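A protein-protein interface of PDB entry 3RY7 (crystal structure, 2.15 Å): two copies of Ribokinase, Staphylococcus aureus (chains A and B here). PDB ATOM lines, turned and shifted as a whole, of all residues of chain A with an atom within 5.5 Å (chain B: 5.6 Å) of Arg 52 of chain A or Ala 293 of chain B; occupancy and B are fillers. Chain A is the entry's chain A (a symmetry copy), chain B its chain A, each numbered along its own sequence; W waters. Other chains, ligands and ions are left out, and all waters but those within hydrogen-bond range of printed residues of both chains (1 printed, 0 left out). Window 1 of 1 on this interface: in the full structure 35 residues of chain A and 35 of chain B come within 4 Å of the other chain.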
ATOM      1  N   ALA A  47     -16.699   7.377  15.341  1.00  0.00           N
ATOM      2  CA  ALA A  47     -15.362   6.949  14.946  1.00  0.00           C
ATOM      3  C   ALA A  47     -14.739   6.022  15.997  1.00  0.00           C
ATOM      4  O   ALA A  47     -14.184   4.980  15.669  1.00  0.00           O
ATOM      5  CB  ALA A  47     -14.469   8.161  14.702  1.00  0.00           C
ATOM      6  N   ILE A  48     -14.827   6.417  17.264  1.00  0.00           N
ATOM      7  CA  ILE A  48     -14.296   5.609  18.353  1.00  0.00           C
ATOM      8  C   ILE A  48     -15.067   4.290  18.479  1.00  0.00           C
ATOM      9  O   ILE A  48     -14.477   3.252  18.722  1.00  0.00           O
ATOM     10  CB  ILE A  48     -14.338   6.370  19.701  1.00  0.00           C
ATOM     11  CG1 ILE A  48     -13.239   7.442  19.737  1.00  0.00           C
ATOM     12  CG2 ILE A  48     -14.199   5.391  20.879  1.00  0.00           C
ATOM     13  CD1 ILE A  48     -13.487   8.539  20.765  1.00  0.00           C
ATOM     14  N   ALA A  49     -16.385   4.333  18.292  1.00  0.00           N
ATOM     15  CA  ALA A  49     -17.180   3.101  18.291  1.00  0.00           C
ATOM     16  C   ALA A  49     -16.748   2.144  17.180  1.00  0.00           C
ATOM     17  O   ALA A  49     -16.410   0.991  17.458  1.00  0.00           O
ATOM     18  CB  ALA A  49     -18.676   3.418  18.200  1.00  0.00           C
ATOM     19  N   THR A  50     -16.742   2.605  15.927  1.00  0.00           N
ATOM     20  CA  THR A  50     -16.383   1.696  14.840  1.00  0.00           C
ATOM     21  C   THR A  50     -14.971   1.157  15.056  1.00  0.00           C
ATOM     22  O   THR A  50     -14.705  -0.018  14.799  1.00  0.00           O
ATOM     23  CB  THR A  50     -16.483   2.337  13.417  1.00  0.00           C
ATOM     24  OG1 THR A  50     -15.312   3.117  13.154  1.00  0.00           O
ATOM     25  CG2 THR A  50     -17.690   3.212  13.302  1.00  0.00           C
ATOM     26  N   ALA A  51     -14.074   2.012  15.542  1.00  0.00           N
ATOM     27  CA  ALA A  51     -12.681   1.610  15.761  1.00  0.00           C
ATOM     28  C   ALA A  51     -12.522   0.615  16.929  1.00  0.00           C
ATOM     29  O   ALA A  51     -11.705  -0.300  16.875  1.00  0.00           O
ATOM     30  CB  ALA A  51     -11.800   2.837  15.968  1.00  0.00           C
ATOM     31  N   ARG A  52     -13.307   0.797  17.983  1.00  0.00           N
ATOM     32  CA  ARG A  52     -13.272  -0.154  19.093  1.00  0.00           C
ATOM     33  C   ARG A  52     -13.921  -1.472  18.693  1.00  0.00           C
ATOM     34  O   ARG A  52     -13.653  -2.503  19.302  1.00  0.00           O
ATOM     35  CB  ARG A  52     -13.895   0.420  20.369  1.00  0.00           C
ATOM     36  CG  ARG A  52     -12.896   1.252  21.176  1.00  0.00           C
ATOM     37  CD  ARG A  52     -13.501   1.951  22.391  1.00  0.00           C
ATOM     38  NE  ARG A  52     -12.573   2.971  22.879  1.00  0.00           N
ATOM     39  CZ  ARG A  52     -12.903   3.979  23.682  1.00  0.00           C
ATOM     40  NH1 ARG A  52     -14.153   4.108  24.132  1.00  0.00           N
ATOM     41  NH2 ARG A  52     -11.973   4.861  24.042  1.00  0.00           N
ATOM     42  N   MET A  53     -14.752  -1.436  17.653  1.00  0.00           N
ATOM     43  CA  MET A  53     -15.293  -2.659  17.069  1.00  0.00           C
ATOM     44  C   MET A  53     -14.296  -3.276  16.099  1.00  0.00           C
ATOM     45  O   MET A  53     -14.607  -4.241  15.418  1.00  0.00           O
ATOM     46  CB  MET A  53     -16.604  -2.370  16.344  1.00  0.00           C
ATOM     47  CG  MET A  53     -17.758  -2.097  17.275  1.00  0.00           C
ATOM     48  SD  MET A  53     -17.559  -3.126  18.733  1.00  0.00           S
ATOM     49  CE  MET A  53     -19.120  -2.885  19.539  1.00  0.00           C
ATOM     50  N   GLN A  54     -13.107  -2.684  16.023  1.00  0.00           N
ATOM     51  CA  GLN A  54     -11.999  -3.194  15.211  1.00  0.00           C
ATOM     52  C   GLN A  54     -12.158  -3.060  13.682  1.00  0.00           C
ATOM     53  O   GLN A  54     -11.471  -3.732  12.907  1.00  0.00           O
ATOM     54  CB  GLN A  54     -11.645  -4.620  15.622  1.00  0.00           C
ATOM     55  CG  GLN A  54     -11.389  -4.721  17.114  1.00  0.00           C
ATOM     56  CD  GLN A  54     -10.641  -5.982  17.505  1.00  0.00           C
ATOM     57  OE1 GLN A  54      -9.925  -6.578  16.692  1.00  0.00           O
ATOM     58  NE2 GLN A  54     -10.796  -6.392  18.763  1.00  0.00           N
ATOM     59  N   ASP A  75      -6.964   9.929  22.474  1.00  0.00           N
ATOM     60  CA  ASP A  75      -7.898   8.812  22.522  1.00  0.00           C
ATOM     61  C   ASP A  75      -8.067   8.186  21.142  1.00  0.00           C
ATOM     62  O   ASP A  75      -8.178   6.960  21.022  1.00  0.00           O
ATOM     63  CB  ASP A  75      -9.238   9.242  23.120  1.00  0.00           C
ATOM     64  CG  ASP A  75      -9.140   9.526  24.609  1.00  0.00           C
ATOM     65  OD1 ASP A  75      -8.357   8.830  25.287  1.00  0.00           O
ATOM     66  OD2 ASP A  75      -9.830  10.450  25.097  1.00  0.00           O
ATOM     67  N   ALA A  79      -7.091   4.264  20.062  1.00  0.00           N
ATOM     68  CA  ALA A  79      -8.061   3.401  19.395  1.00  0.00           C
ATOM     69  C   ALA A  79      -7.578   2.955  18.014  1.00  0.00           C
ATOM     70  O   ALA A  79      -8.250   2.198  17.327  1.00  0.00           O
ATOM     71  CB  ALA A  79      -9.412   4.086  19.307  1.00  0.00           C
ATOM     72  N   HIS B 289     -16.736   9.590  34.179  1.00  0.00           N
ATOM     73  CA  HIS B 289     -15.755   9.257  33.144  1.00  0.00           C
ATOM     74  C   HIS B 289     -16.088   9.780  31.729  1.00  0.00           C
ATOM     75  O   HIS B 289     -15.194   9.937  30.884  1.00  0.00           O
ATOM     76  CB  HIS B 289     -15.494   7.752  33.130  1.00  0.00           C
ATOM     77  CG  HIS B 289     -14.895   7.245  34.400  1.00  0.00           C
ATOM     78  ND1 HIS B 289     -13.638   7.630  34.834  1.00  0.00           N
ATOM     79  CD2 HIS B 289     -15.373   6.404  35.346  1.00  0.00           C
ATOM     80  CE1 HIS B 289     -13.372   7.044  35.984  1.00  0.00           C
ATOM     81  NE2 HIS B 289     -14.412   6.291  36.320  1.00  0.00           N
ATOM     82  N   GLY B 290     -17.363  10.062  31.478  1.00  0.00           N
ATOM     83  CA  GLY B 290     -17.756  10.595  30.191  1.00  0.00           C
ATOM     84  C   GLY B 290     -18.205   9.527  29.213  1.00  0.00           C
ATOM     85  O   GLY B 290     -17.790   8.365  29.288  1.00  0.00           O
ATOM     86  N   ALA B 291     -19.052   9.932  28.275  1.00  0.00           N
ATOM     87  CA  ALA B 291     -19.635   8.999  27.319  1.00  0.00           C
ATOM     88  C   ALA B 291     -18.616   8.236  26.449  1.00  0.00           C
ATOM     89  O   ALA B 291     -18.686   7.014  26.357  1.00  0.00           O
ATOM     90  CB  ALA B 291     -20.661   9.719  26.455  1.00  0.00           C
ATOM     91  N   GLN B 292     -17.674   8.938  25.816  1.00  0.00           N
ATOM     92  CA  GLN B 292     -16.744   8.268  24.902  1.00  0.00           C
ATOM     93  C   GLN B 292     -15.976   7.190  25.614  1.00  0.00           C
ATOM     94  O   GLN B 292     -15.627   6.166  25.023  1.00  0.00           O
ATOM     95  CB  GLN B 292     -15.743   9.237  24.283  1.00  0.00           C
ATOM     96  CG  GLN B 292     -16.374  10.246  23.413  1.00  0.00           C
ATOM     97  CD  GLN B 292     -15.374  10.988  22.575  1.00  0.00           C
ATOM     98  OE1 GLN B 292     -14.214  11.193  22.967  1.00  0.00           O
ATOM     99  NE2 GLN B 292     -15.810  11.396  21.396  1.00  0.00           N
ATOM    100  N   ALA B 293     -15.704   7.444  26.890  1.00  0.00           N
ATOM    101  CA  ALA B 293     -14.887   6.559  27.701  1.00  0.00           C
ATOM    102  C   ALA B 293     -15.564   5.203  27.869  1.00  0.00           C
ATOM    103  O   ALA B 293     -14.903   4.176  28.013  1.00  0.00           O
ATOM    104  CB  ALA B 293     -14.629   7.206  29.064  1.00  0.00           C
ATOM    105  N   SER B 294     -16.890   5.210  27.870  1.00  0.00           N
ATOM    106  CA  SER B 294     -17.636   3.980  28.063  1.00  0.00           C
ATOM    107  C   SER B 294     -18.158   3.360  26.766  1.00  0.00           C
ATOM    108  O   SER B 294     -18.939   2.410  26.795  1.00  0.00           O
ATOM    109  CB  SER B 294     -18.755   4.188  29.075  1.00  0.00           C
ATOM    110  OG  SER B 294     -18.227   4.574  30.333  1.00  0.00           O
ATOM    111  N   ILE B 295     -17.736   3.912  25.631  1.00  0.00           N
ATOM    112  CA  ILE B 295     -17.995   3.247  24.358  1.00  0.00           C
ATOM    113  C   ILE B 295     -17.177   1.957  24.375  1.00  0.00           C
ATOM    114  O   ILE B 295     -15.943   1.997  24.463  1.00  0.00           O
ATOM    115  CB  ILE B 295     -17.639   4.121  23.125  1.00  0.00           C
ATOM    116  CG1 ILE B 295     -18.599   5.307  23.023  1.00  0.00           C
ATOM    117  CG2 ILE B 295     -17.674   3.306  21.849  1.00  0.00           C
ATOM    118  CD1 ILE B 295     -18.232   6.308  21.933  1.00  0.00           C
ATOM    119  N   PRO B 296     -17.873   0.803  24.292  1.00  0.00           N
ATOM    120  CA  PRO B 296     -17.344  -0.564  24.474  1.00  0.00           C
ATOM    121  C   PRO B 296     -16.340  -1.072  23.430  1.00  0.00           C
ATOM    122  O   PRO B 296     -16.248  -0.568  22.306  1.00  0.00           O
ATOM    123  CB  PRO B 296     -18.607  -1.442  24.448  1.00  0.00           C
ATOM    124  CG  PRO B 296     -19.635  -0.630  23.694  1.00  0.00           C
ATOM    125  CD  PRO B 296     -19.328   0.810  24.038  1.00  0.00           C
ATOM    126  N   LEU B 297     -15.582  -2.090  23.828  1.00  0.00           N
ATOM    127  CA  LEU B 297     -14.667  -2.776  22.929  1.00  0.00           C
ATOM    128  C   LEU B 297     -15.333  -4.034  22.357  1.00  0.00           C
ATOM    129  O   LEU B 297     -16.271  -4.576  22.943  1.00  0.00           O
ATOM    130  CB  LEU B 297     -13.381  -3.159  23.667  1.00  0.00           C
ATOM    131  CG  LEU B 297     -12.517  -2.059  24.276  1.00  0.00           C
ATOM    132  CD1 LEU B 297     -11.624  -2.660  25.358  1.00  0.00           C
ATOM    133  CD2 LEU B 297     -11.689  -1.371  23.200  1.00  0.00           C
ATOM    134  N   LEU B 298     -14.845  -4.487  21.206  1.00  0.00           N
ATOM    135  CA  LEU B 298     -15.344  -5.706  20.577  1.00  0.00           C
ATOM    136  C   LEU B 298     -15.506  -6.848  21.596  1.00  0.00           C
ATOM    137  O   LEU B 298     -16.572  -7.481  21.674  1.00  0.00           O
ATOM    138  CB  LEU B 298     -14.380  -6.140  19.471  1.00  0.00           C
ATOM    139  CG  LEU B 298     -14.942  -6.899  18.274  1.00  0.00           C
ATOM    140  CD1 LEU B 298     -13.887  -7.853  17.725  1.00  0.00           C
ATOM    141  CD2 LEU B 298     -16.242  -7.621  18.619  1.00  0.00           C
HETATM  142  O   HOH W   1     -12.455  10.586  24.883  1.00  0.00           O
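The backbone carbonyl oxygen of Gln 292 of chain B sits at hydrogen-bond distance from the guanidinium group of Arg 52 of chain A (2.7 Å). The guanidinium group of Arg 52 of chain A sits at hydrogen-bond distance from the backbone carbonyl oxygen of Ile 295 of chain B (2.8 Å). O of Arg 52 of chain A lies within hydrogen-bond range of N of Leu 298 of chain B, 3.0 Å away.
Among the printed residues, pairs that only touch across the chains: Ile 48 of chain A with Gln 292 of chain B (3.5 Å), Ala 49 of chain A with Ile 295 of chain B (3.6 Å), Arg 52 of chain A with Ala 293 of chain B (3.95 Å), Arg 52 of chain A with Pro 296 of chain B (3.2 Å), Arg 52 of chain A with Leu 297 of chain B (3.5 Å), Met 53 of chain A with Leu 298 of chain B (3.9 Å) and Gln 54 of chain A with Leu 298 of chain B (3.6 Å).
Arg 52 of chain A touches just these residues of chain B: Gln 292 (2.7 Å), Ala 293 (3.95 Å), Ile 295 (2.8 Å), Pro 296 (3.2 Å), Leu 297 (3.5 Å) and Leu 298 (3.0 Å). Gly 290 of chain B touches none of the printed residues of chain A. Ala 293 of chain B touches just one residue of chain A: Arg 52. Of the printed residues of chain A, Pro 296 of chain B touches Arg 52 (3.2 Å). Of the printed residues of chain A, Leu 297 of chain B touches Arg 52. The nearest printed residue of chain B that does not touch Ile 48 of chain A is Ile 295 of chain B (4.2 Å).
Of the 10 printed residues of chain A, 5 touch a printed residue of chain B. Printed residues of chain A that touch a printed residue of chain B: Ile 48, Ala 49, Arg 52, Met 53 and Gln 54. Hydrophobic or aromatic side chains of chain A that line the printed part of chain B: Ile 48, Ala 49 and Met 53. Along chain A the printed residues that touch a printed residue of chain B span positions 48 to 54. Printed residues of chain B that touch a printed residue of chain A: Gln 292, Ala 293, Ile 295, Pro 296, Leu 297 and Leu 298. Hydrophobic or aromatic side chains of chain B that line the printed part of chain A: Ile 295, Leu 297 and Leu 298. Among the printed residues, 10 pairs touch across the chains.
No position is printed for both chains. Of the 10 pairs that touch across the chains among the printed residues, none has its exchanged pair printed and touching as well.
Water W1 bridges OD2 of Asp 75 of chain A (2.6 Å) and OE1 of Gln 292 of chain B (2.7 Å).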
